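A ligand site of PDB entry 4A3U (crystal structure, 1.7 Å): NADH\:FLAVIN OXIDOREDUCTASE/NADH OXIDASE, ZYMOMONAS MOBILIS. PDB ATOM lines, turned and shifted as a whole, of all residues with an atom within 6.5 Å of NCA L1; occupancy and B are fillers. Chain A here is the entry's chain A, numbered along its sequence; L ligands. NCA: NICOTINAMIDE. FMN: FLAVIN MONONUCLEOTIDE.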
ATOM      1  N   PRO A  23      -6.172  21.670  23.598  1.00  0.00           N
ATOM      2  CA  PRO A  23      -5.001  21.876  24.454  1.00  0.00           C
ATOM      3  C   PRO A  23      -5.325  22.108  25.929  1.00  0.00           C
ATOM      4  O   PRO A  23      -6.075  23.034  26.281  1.00  0.00           O
ATOM      5  CB  PRO A  23      -4.328  23.117  23.870  1.00  0.00           C
ATOM      6  CG  PRO A  23      -5.429  23.817  23.082  1.00  0.00           C
ATOM      7  CD  PRO A  23      -6.392  22.794  22.649  1.00  0.00           C
ATOM      8  N   LEU A  24      -4.741  21.274  26.789  1.00  0.00           N
ATOM      9  CA  LEU A  24      -5.002  21.290  28.244  1.00  0.00           C
ATOM     10  C   LEU A  24      -3.708  21.282  29.083  1.00  0.00           C
ATOM     11  O   LEU A  24      -3.024  20.259  29.093  1.00  0.00           O
ATOM     12  CB  LEU A  24      -5.867  20.085  28.586  1.00  0.00           C
ATOM     13  CG  LEU A  24      -7.335  20.207  28.075  1.00  0.00           C
ATOM     14  CD1 LEU A  24      -7.968  18.825  27.857  1.00  0.00           C
ATOM     15  CD2 LEU A  24      -8.254  21.104  28.909  1.00  0.00           C
ATOM     16  N   THR A  25      -3.353  22.420  29.724  1.00  0.00           N
ATOM     17  CA  THR A  25      -2.150  22.537  30.591  1.00  0.00           C
ATOM     18  C   THR A  25      -2.479  21.729  31.842  1.00  0.00           C
ATOM     19  O   THR A  25      -3.481  21.990  32.465  1.00  0.00           O
ATOM     20  CB  THR A  25      -1.828  23.988  30.932  1.00  0.00           C
ATOM     21  OG1 THR A  25      -1.294  24.603  29.769  1.00  0.00           O
ATOM     22  CG2 THR A  25      -0.749  24.161  32.090  1.00  0.00           C
ATOM     23  N   ALA A  56      -0.058  23.128  26.411  1.00  0.00           N
ATOM     24  CA  ALA A  56       0.792  24.211  25.926  1.00  0.00           C
ATOM     25  C   ALA A  56       2.224  23.894  26.247  1.00  0.00           C
ATOM     26  O   ALA A  56       2.515  23.555  27.381  1.00  0.00           O
ATOM     27  CB  ALA A  56       0.363  25.538  26.544  1.00  0.00           C
ATOM     28  N   TRP A  66       4.856  28.694  33.159  1.00  0.00           N
ATOM     29  CA  TRP A  66       3.853  27.899  33.848  1.00  0.00           C
ATOM     30  C   TRP A  66       4.520  26.802  34.590  1.00  0.00           C
ATOM     31  O   TRP A  66       5.187  25.968  33.971  1.00  0.00           O
ATOM     32  CB  TRP A  66       2.789  27.326  32.904  1.00  0.00           C
ATOM     33  CG  TRP A  66       1.613  26.754  33.662  1.00  0.00           C
ATOM     34  CD1 TRP A  66       1.575  25.560  34.392  1.00  0.00           C
ATOM     35  CD2 TRP A  66       0.311  27.387  33.909  1.00  0.00           C
ATOM     36  NE1 TRP A  66       0.375  25.414  35.027  1.00  0.00           N
ATOM     37  CE2 TRP A  66      -0.438  26.459  34.740  1.00  0.00           C
ATOM     38  CE3 TRP A  66      -0.308  28.566  33.464  1.00  0.00           C
ATOM     39  CZ2 TRP A  66      -1.729  26.736  35.170  1.00  0.00           C
ATOM     40  CZ3 TRP A  66      -1.589  28.844  33.904  1.00  0.00           C
ATOM     41  CH2 TRP A  66      -2.304  27.937  34.712  1.00  0.00           C
ATOM     42  N   GLN A  98       1.246  22.038  20.938  1.00  0.00           N
ATOM     43  CA  GLN A  98       0.960  23.484  21.049  1.00  0.00           C
ATOM     44  C   GLN A  98       2.217  24.243  21.453  1.00  0.00           C
ATOM     45  O   GLN A  98       2.802  24.003  22.469  1.00  0.00           O
ATOM     46  CB  GLN A  98      -0.179  23.773  22.052  1.00  0.00           C
ATOM     47  CG  GLN A  98      -0.950  25.020  21.667  1.00  0.00           C
ATOM     48  CD  GLN A  98      -1.940  25.504  22.723  1.00  0.00           C
ATOM     49  OE1 GLN A  98      -1.757  25.323  23.944  1.00  0.00           O
ATOM     50  NE2 GLN A  98      -3.035  26.099  22.236  1.00  0.00           N
ATOM     51  N   TRP A 100       4.252  27.467  22.596  1.00  0.00           N
ATOM     52  CA  TRP A 100       3.801  28.398  23.657  1.00  0.00           C
ATOM     53  C   TRP A 100       4.841  29.393  23.998  1.00  0.00           C
ATOM     54  O   TRP A 100       6.004  29.019  24.352  1.00  0.00           O
ATOM     55  CB  TRP A 100       3.435  27.643  24.964  1.00  0.00           C
ATOM     56  CG  TRP A 100       2.374  28.279  25.848  1.00  0.00           C
ATOM     57  CD1 TRP A 100       1.417  29.204  25.484  1.00  0.00           C
ATOM     58  CD2 TRP A 100       2.046  27.910  27.255  1.00  0.00           C
ATOM     59  NE1 TRP A 100       0.612  29.510  26.542  1.00  0.00           N
ATOM     60  CE2 TRP A 100       0.925  28.753  27.621  1.00  0.00           C
ATOM     61  CE3 TRP A 100       2.592  27.032  28.201  1.00  0.00           C
ATOM     62  CZ2 TRP A 100       0.341  28.688  28.887  1.00  0.00           C
ATOM     63  CZ3 TRP A 100       1.985  26.951  29.451  1.00  0.00           C
ATOM     64  CH2 TRP A 100       0.912  27.769  29.805  1.00  0.00           C
ATOM     65  N   HIS A 172       0.299  28.773  19.603  1.00  0.00           N
ATOM     66  CA  HIS A 172      -0.579  29.394  20.603  1.00  0.00           C
ATOM     67  C   HIS A 172      -0.604  30.889  20.384  1.00  0.00           C
ATOM     68  O   HIS A 172       0.369  31.597  20.713  1.00  0.00           O
ATOM     69  CB  HIS A 172      -0.132  29.049  22.017  1.00  0.00           C
ATOM     70  CG  HIS A 172      -1.244  29.161  23.017  1.00  0.00           C
ATOM     71  ND1 HIS A 172      -2.287  30.024  22.878  1.00  0.00           N
ATOM     72  CD2 HIS A 172      -1.456  28.480  24.189  1.00  0.00           C
ATOM     73  CE1 HIS A 172      -3.092  29.875  23.913  1.00  0.00           C
ATOM     74  NE2 HIS A 172      -2.576  28.960  24.710  1.00  0.00           N
ATOM     75  N   ALA A 174      -3.762  32.491  21.211  1.00  0.00           N
ATOM     76  CA  ALA A 174      -4.920  32.918  22.064  1.00  0.00           C
ATOM     77  C   ALA A 174      -4.617  33.217  23.492  1.00  0.00           C
ATOM     78  O   ALA A 174      -3.434  33.152  23.906  1.00  0.00           O
ATOM     79  CB  ALA A 174      -5.988  31.880  22.045  1.00  0.00           C
ATOM     80  N   ASN A 175      -5.701  33.602  24.190  1.00  0.00           N
ATOM     81  CA  ASN A 175      -5.868  33.486  25.625  1.00  0.00           C
ATOM     82  C   ASN A 175      -5.009  34.468  26.371  1.00  0.00           C
ATOM     83  O   ASN A 175      -4.777  34.319  27.544  1.00  0.00           O
ATOM     84  CB  ASN A 175      -5.747  32.022  26.095  1.00  0.00           C
ATOM     85  CG  ASN A 175      -6.861  31.128  25.477  1.00  0.00           C
ATOM     86  OD1 ASN A 175      -7.752  31.598  24.825  1.00  0.00           O
ATOM     87  ND2 ASN A 175      -6.749  29.816  25.645  1.00  0.00           N
ATOM     88  N   TYR A 177      -1.792  35.396  25.753  1.00  0.00           N
ATOM     89  CA  TYR A 177      -0.363  35.182  25.743  1.00  0.00           C
ATOM     90  C   TYR A 177       0.274  36.070  24.646  1.00  0.00           C
ATOM     91  O   TYR A 177      -0.357  37.058  24.244  1.00  0.00           O
ATOM     92  CB  TYR A 177      -0.043  33.671  25.648  1.00  0.00           C
ATOM     93  CG  TYR A 177      -0.568  32.941  26.864  1.00  0.00           C
ATOM     94  CD1 TYR A 177      -0.028  33.206  28.107  1.00  0.00           C
ATOM     95  CD2 TYR A 177      -1.644  32.048  26.789  1.00  0.00           C
ATOM     96  CE1 TYR A 177      -0.496  32.573  29.242  1.00  0.00           C
ATOM     97  CE2 TYR A 177      -2.129  31.398  27.932  1.00  0.00           C
ATOM     98  CZ  TYR A 177      -1.544  31.664  29.144  1.00  0.00           C
ATOM     99  OH  TYR A 177      -1.972  31.032  30.293  1.00  0.00           O
ATOM    100  N   ARG A 224      -3.970  28.621  16.899  1.00  0.00           N
ATOM    101  CA  ARG A 224      -5.049  28.981  17.774  1.00  0.00           C
ATOM    102  C   ARG A 224      -5.216  30.476  17.982  1.00  0.00           C
ATOM    103  O   ARG A 224      -4.265  31.157  18.353  1.00  0.00           O
ATOM    104  CB  ARG A 224      -4.925  28.317  19.159  1.00  0.00           C
ATOM    105  CG  ARG A 224      -6.310  27.941  19.701  1.00  0.00           C
ATOM    106  CD  ARG A 224      -6.169  27.294  21.078  1.00  0.00           C
ATOM    107  NE  ARG A 224      -7.306  26.466  21.436  1.00  0.00           N
ATOM    108  CZ  ARG A 224      -7.806  26.327  22.665  1.00  0.00           C
ATOM    109  NH1 ARG A 224      -7.366  27.031  23.717  1.00  0.00           N
ATOM    110  NH2 ARG A 224      -8.824  25.498  22.843  1.00  0.00           N
ATOM    111  N   ILE A 231      -9.593  38.249  28.326  1.00  0.00           N
ATOM    112  CA  ILE A 231      -8.837  37.187  29.033  1.00  0.00           C
ATOM    113  C   ILE A 231      -7.453  37.636  29.438  1.00  0.00           C
ATOM    114  O   ILE A 231      -6.586  37.979  28.609  1.00  0.00           O
ATOM    115  CB  ILE A 231      -8.795  35.862  28.197  1.00  0.00           C
ATOM    116  CG1 ILE A 231      -8.127  34.687  28.958  1.00  0.00           C
ATOM    117  CG2 ILE A 231      -8.175  36.113  26.850  1.00  0.00           C
ATOM    118  CD1 ILE A 231      -8.862  34.224  30.185  1.00  0.00           C
ATOM    119  N   GLN A 232      -7.185  37.550  30.752  1.00  0.00           N
ATOM    120  CA  GLN A 232      -5.876  37.985  31.281  1.00  0.00           C
ATOM    121  C   GLN A 232      -5.419  39.423  30.816  1.00  0.00           C
ATOM    122  O   GLN A 232      -4.283  39.634  30.456  1.00  0.00           O
ATOM    123  CB  GLN A 232      -4.805  36.948  30.916  1.00  0.00           C
ATOM    124  CG  GLN A 232      -5.159  35.528  31.289  1.00  0.00           C
ATOM    125  CD  GLN A 232      -4.007  34.583  31.030  1.00  0.00           C
ATOM    126  OE1 GLN A 232      -3.751  34.144  29.884  1.00  0.00           O
ATOM    127  NE2 GLN A 232      -3.271  34.283  32.100  1.00  0.00           N
ATOM    128  N   ARG A 261     -11.100  29.145  20.419  1.00  0.00           N
ATOM    129  CA  ARG A 261     -11.947  29.082  21.604  1.00  0.00           C
ATOM    130  C   ARG A 261     -12.841  30.311  21.612  1.00  0.00           C
ATOM    131  O   ARG A 261     -12.332  31.434  21.610  1.00  0.00           O
ATOM    132  CB  ARG A 261     -11.056  29.128  22.856  1.00  0.00           C
ATOM    133  CG  ARG A 261     -11.837  29.176  24.168  1.00  0.00           C
ATOM    134  CD  ARG A 261     -11.025  29.471  25.433  1.00  0.00           C
ATOM    135  NE  ARG A 261     -10.475  30.814  25.455  1.00  0.00           N
ATOM    136  CZ  ARG A 261     -11.153  31.966  25.556  1.00  0.00           C
ATOM    137  NH1 ARG A 261     -12.466  31.992  25.799  1.00  0.00           N
ATOM    138  NH2 ARG A 261     -10.485  33.104  25.517  1.00  0.00           N
ATOM    139  N   PHE A 269     -15.682  28.999  30.301  1.00  0.00           N
ATOM    140  CA  PHE A 269     -14.228  29.269  30.259  1.00  0.00           C
ATOM    141  C   PHE A 269     -13.917  30.551  29.477  1.00  0.00           C
ATOM    142  O   PHE A 269     -12.973  30.600  28.681  1.00  0.00           O
ATOM    143  CB  PHE A 269     -13.422  28.068  29.711  1.00  0.00           C
ATOM    144  CG  PHE A 269     -12.073  27.939  30.355  1.00  0.00           C
ATOM    145  CD1 PHE A 269     -10.952  28.599  29.833  1.00  0.00           C
ATOM    146  CD2 PHE A 269     -11.918  27.175  31.517  1.00  0.00           C
ATOM    147  CE1 PHE A 269      -9.699  28.482  30.419  1.00  0.00           C
ATOM    148  CE2 PHE A 269     -10.678  27.071  32.131  1.00  0.00           C
ATOM    149  CZ  PHE A 269      -9.558  27.715  31.584  1.00  0.00           C
ATOM    150  N   TYR A 343      -4.315  21.122  37.688  1.00  0.00           N
ATOM    151  CA  TYR A 343      -2.937  21.555  37.684  1.00  0.00           C
ATOM    152  C   TYR A 343      -2.106  21.119  38.876  1.00  0.00           C
ATOM    153  O   TYR A 343      -1.044  21.660  39.081  1.00  0.00           O
ATOM    154  CB  TYR A 343      -2.836  23.074  37.674  1.00  0.00           C
ATOM    155  CG  TYR A 343      -3.758  23.805  36.707  1.00  0.00           C
ATOM    156  CD1 TYR A 343      -3.575  23.734  35.346  1.00  0.00           C
ATOM    157  CD2 TYR A 343      -4.769  24.646  37.174  1.00  0.00           C
ATOM    158  CE1 TYR A 343      -4.377  24.443  34.474  1.00  0.00           C
ATOM    159  CE2 TYR A 343      -5.586  25.357  36.297  1.00  0.00           C
ATOM    160  CZ  TYR A 343      -5.406  25.244  34.944  1.00  0.00           C
ATOM    161  OH  TYR A 343      -6.228  25.953  34.081  1.00  0.00           O
HETATM  162  N1  NCA L   1      -2.899  27.024  30.413  1.00  0.00           N
HETATM  163  C2  NCA L   1      -3.287  27.671  29.317  1.00  0.00           C
HETATM  164  C3  NCA L   1      -4.528  28.339  29.289  1.00  0.00           C
HETATM  165  C4  NCA L   1      -5.367  28.331  30.394  1.00  0.00           C
HETATM  166  C5  NCA L   1      -4.932  27.649  31.537  1.00  0.00           C
HETATM  167  C6  NCA L   1      -3.701  27.012  31.514  1.00  0.00           C
HETATM  168  C7  NCA L   1      -5.020  29.103  28.073  1.00  0.00           C
HETATM  169  O7  NCA L   1      -6.114  29.669  28.174  1.00  0.00           O
HETATM  170  N7  NCA L   1      -4.247  29.170  27.001  1.00  0.00           N
HETATM  171  N1  FMN L   2      -5.880  26.407  26.112  1.00  0.00           N
HETATM  172  C2  FMN L   2      -4.739  26.452  25.474  1.00  0.00           C
HETATM  173  O2  FMN L   2      -4.836  27.074  24.391  1.00  0.00           O
HETATM  174  N3  FMN L   2      -3.574  25.870  25.918  1.00  0.00           N
HETATM  175  C4  FMN L   2      -3.562  25.232  27.114  1.00  0.00           C
HETATM  176  O4  FMN L   2      -2.478  24.693  27.464  1.00  0.00           O
HETATM  177  C4A FMN L   2      -4.841  25.140  27.889  1.00  0.00           C
HETATM  178  N5  FMN L   2      -4.929  24.521  29.086  1.00  0.00           N
HETATM  179  C5A FMN L   2      -6.087  24.420  29.793  1.00  0.00           C
HETATM  180  C6  FMN L   2      -6.112  23.718  31.020  1.00  0.00           C
HETATM  181  C7  FMN L   2      -7.293  23.563  31.734  1.00  0.00           C
HETATM  182  C7M FMN L   2      -7.271  22.808  33.021  1.00  0.00           C
HETATM  183  C8  FMN L   2      -8.528  24.175  31.236  1.00  0.00           C
HETATM  184  C8M FMN L   2      -9.784  24.047  32.012  1.00  0.00           C
HETATM  185  C9  FMN L   2      -8.522  24.883  30.033  1.00  0.00           C
HETATM  186  C9A FMN L   2      -7.363  25.014  29.256  1.00  0.00           C
HETATM  187  N10 FMN L   2      -7.299  25.710  27.995  1.00  0.00           N
HETATM  188  C10 FMN L   2      -6.061  25.774  27.308  1.00  0.00           C
HETATM  189  C1' FMN L   2      -8.568  26.270  27.523  1.00  0.00           C
HETATM  190  C2' FMN L   2      -9.230  24.981  26.951  1.00  0.00           C
HETATM  191  O2' FMN L   2      -8.613  24.549  25.762  1.00  0.00           O
HETATM  192  C3' FMN L   2     -10.626  25.118  26.450  1.00  0.00           C
HETATM  193  O3' FMN L   2     -10.514  26.170  25.474  1.00  0.00           O
HETATM  194  C4' FMN L   2     -11.596  25.275  27.576  1.00  0.00           C
HETATM  195  O4' FMN L   2     -11.491  24.055  28.363  1.00  0.00           O
HETATM  196  C5' FMN L   2     -12.985  25.497  26.993  1.00  0.00           C
HETATM  197  O5' FMN L   2     -13.381  24.271  26.379  1.00  0.00           O
HETATM  198  P   FMN L   2     -14.351  23.194  26.969  1.00  0.00           P
HETATM  199  O1P FMN L   2     -13.614  22.600  28.167  1.00  0.00           O
HETATM  200  O2P FMN L   2     -15.587  23.966  27.377  1.00  0.00           O
HETATM  201  O3P FMN L   2     -14.469  22.125  25.903  1.00  0.00           O
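N7 of NCA L1 sits close to N1 of FMN L2, 3.3 Å away.
NE of Arg 261 lies within hydrogen-bond range of OD1 of Asn 175. The guanidinium group (NH1) of Arg 224 sits close to the side-chain amide nitrogen (ND2) of Asn 175, 3.4 Å away. OE1 of Gln 232 sits close to O of Asn 175 (2.6 Å). ND1 of His 172 is in hydrogen-bond range of N of Ala 174, at 3.3 Å.
Residues that only touch NCA L1: Trp 66 (3.6 Å), Trp 100 (3.8 Å), Tyr 177 (3.2 Å) and Tyr 343 (3.3 Å). Hydrophobic or aromatic side chains that line NCA L1: Trp 66, Trp 100, His 172, Tyr 177 and Tyr 343. Of the 17 residues printed, 7 come within 4 Å of NCA L1.
A ring nitrogen (NE2) of His 172 sits at hydrogen-bond distance from an oxygen (O2) of FMN L2. The backbone NH (N) of Thr 25 is in hydrogen-bond range of a nitrogen (N5) of FMN L2 (2.7 Å). The backbone carbonyl oxygen of Pro 23 sits close to an oxygen (O2') of FMN L2 (3.0 Å). The guanidinium group (NH1) of Arg 224 is in hydrogen-bond range of an oxygen (O2) of FMN L2, 2.6 Å away. N7 of NCA L1 lies within hydrogen-bond range of NE2 of His 172, 2.8 Å away. O4 of FMN L2 sits at hydrogen-bond distance from N of Ala 56, at 3.1 Å. The side-chain amide oxygen (OE1) of Gln 98 sits at hydrogen-bond distance from a nitrogen (N3) of FMN L2 (2.7 Å). The side-chain hydroxyl (OG1) of Thr 25 lies within hydrogen-bond range of a nitrogen (N1) of NCA L1. The side-chain hydroxyl of Thr 25 lies within hydrogen-bond range of an oxygen (O4) of FMN L2 (2.6 Å). O7 of NCA L1 sits at hydrogen-bond distance from ND2 of Asn 175 (2.6 Å).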
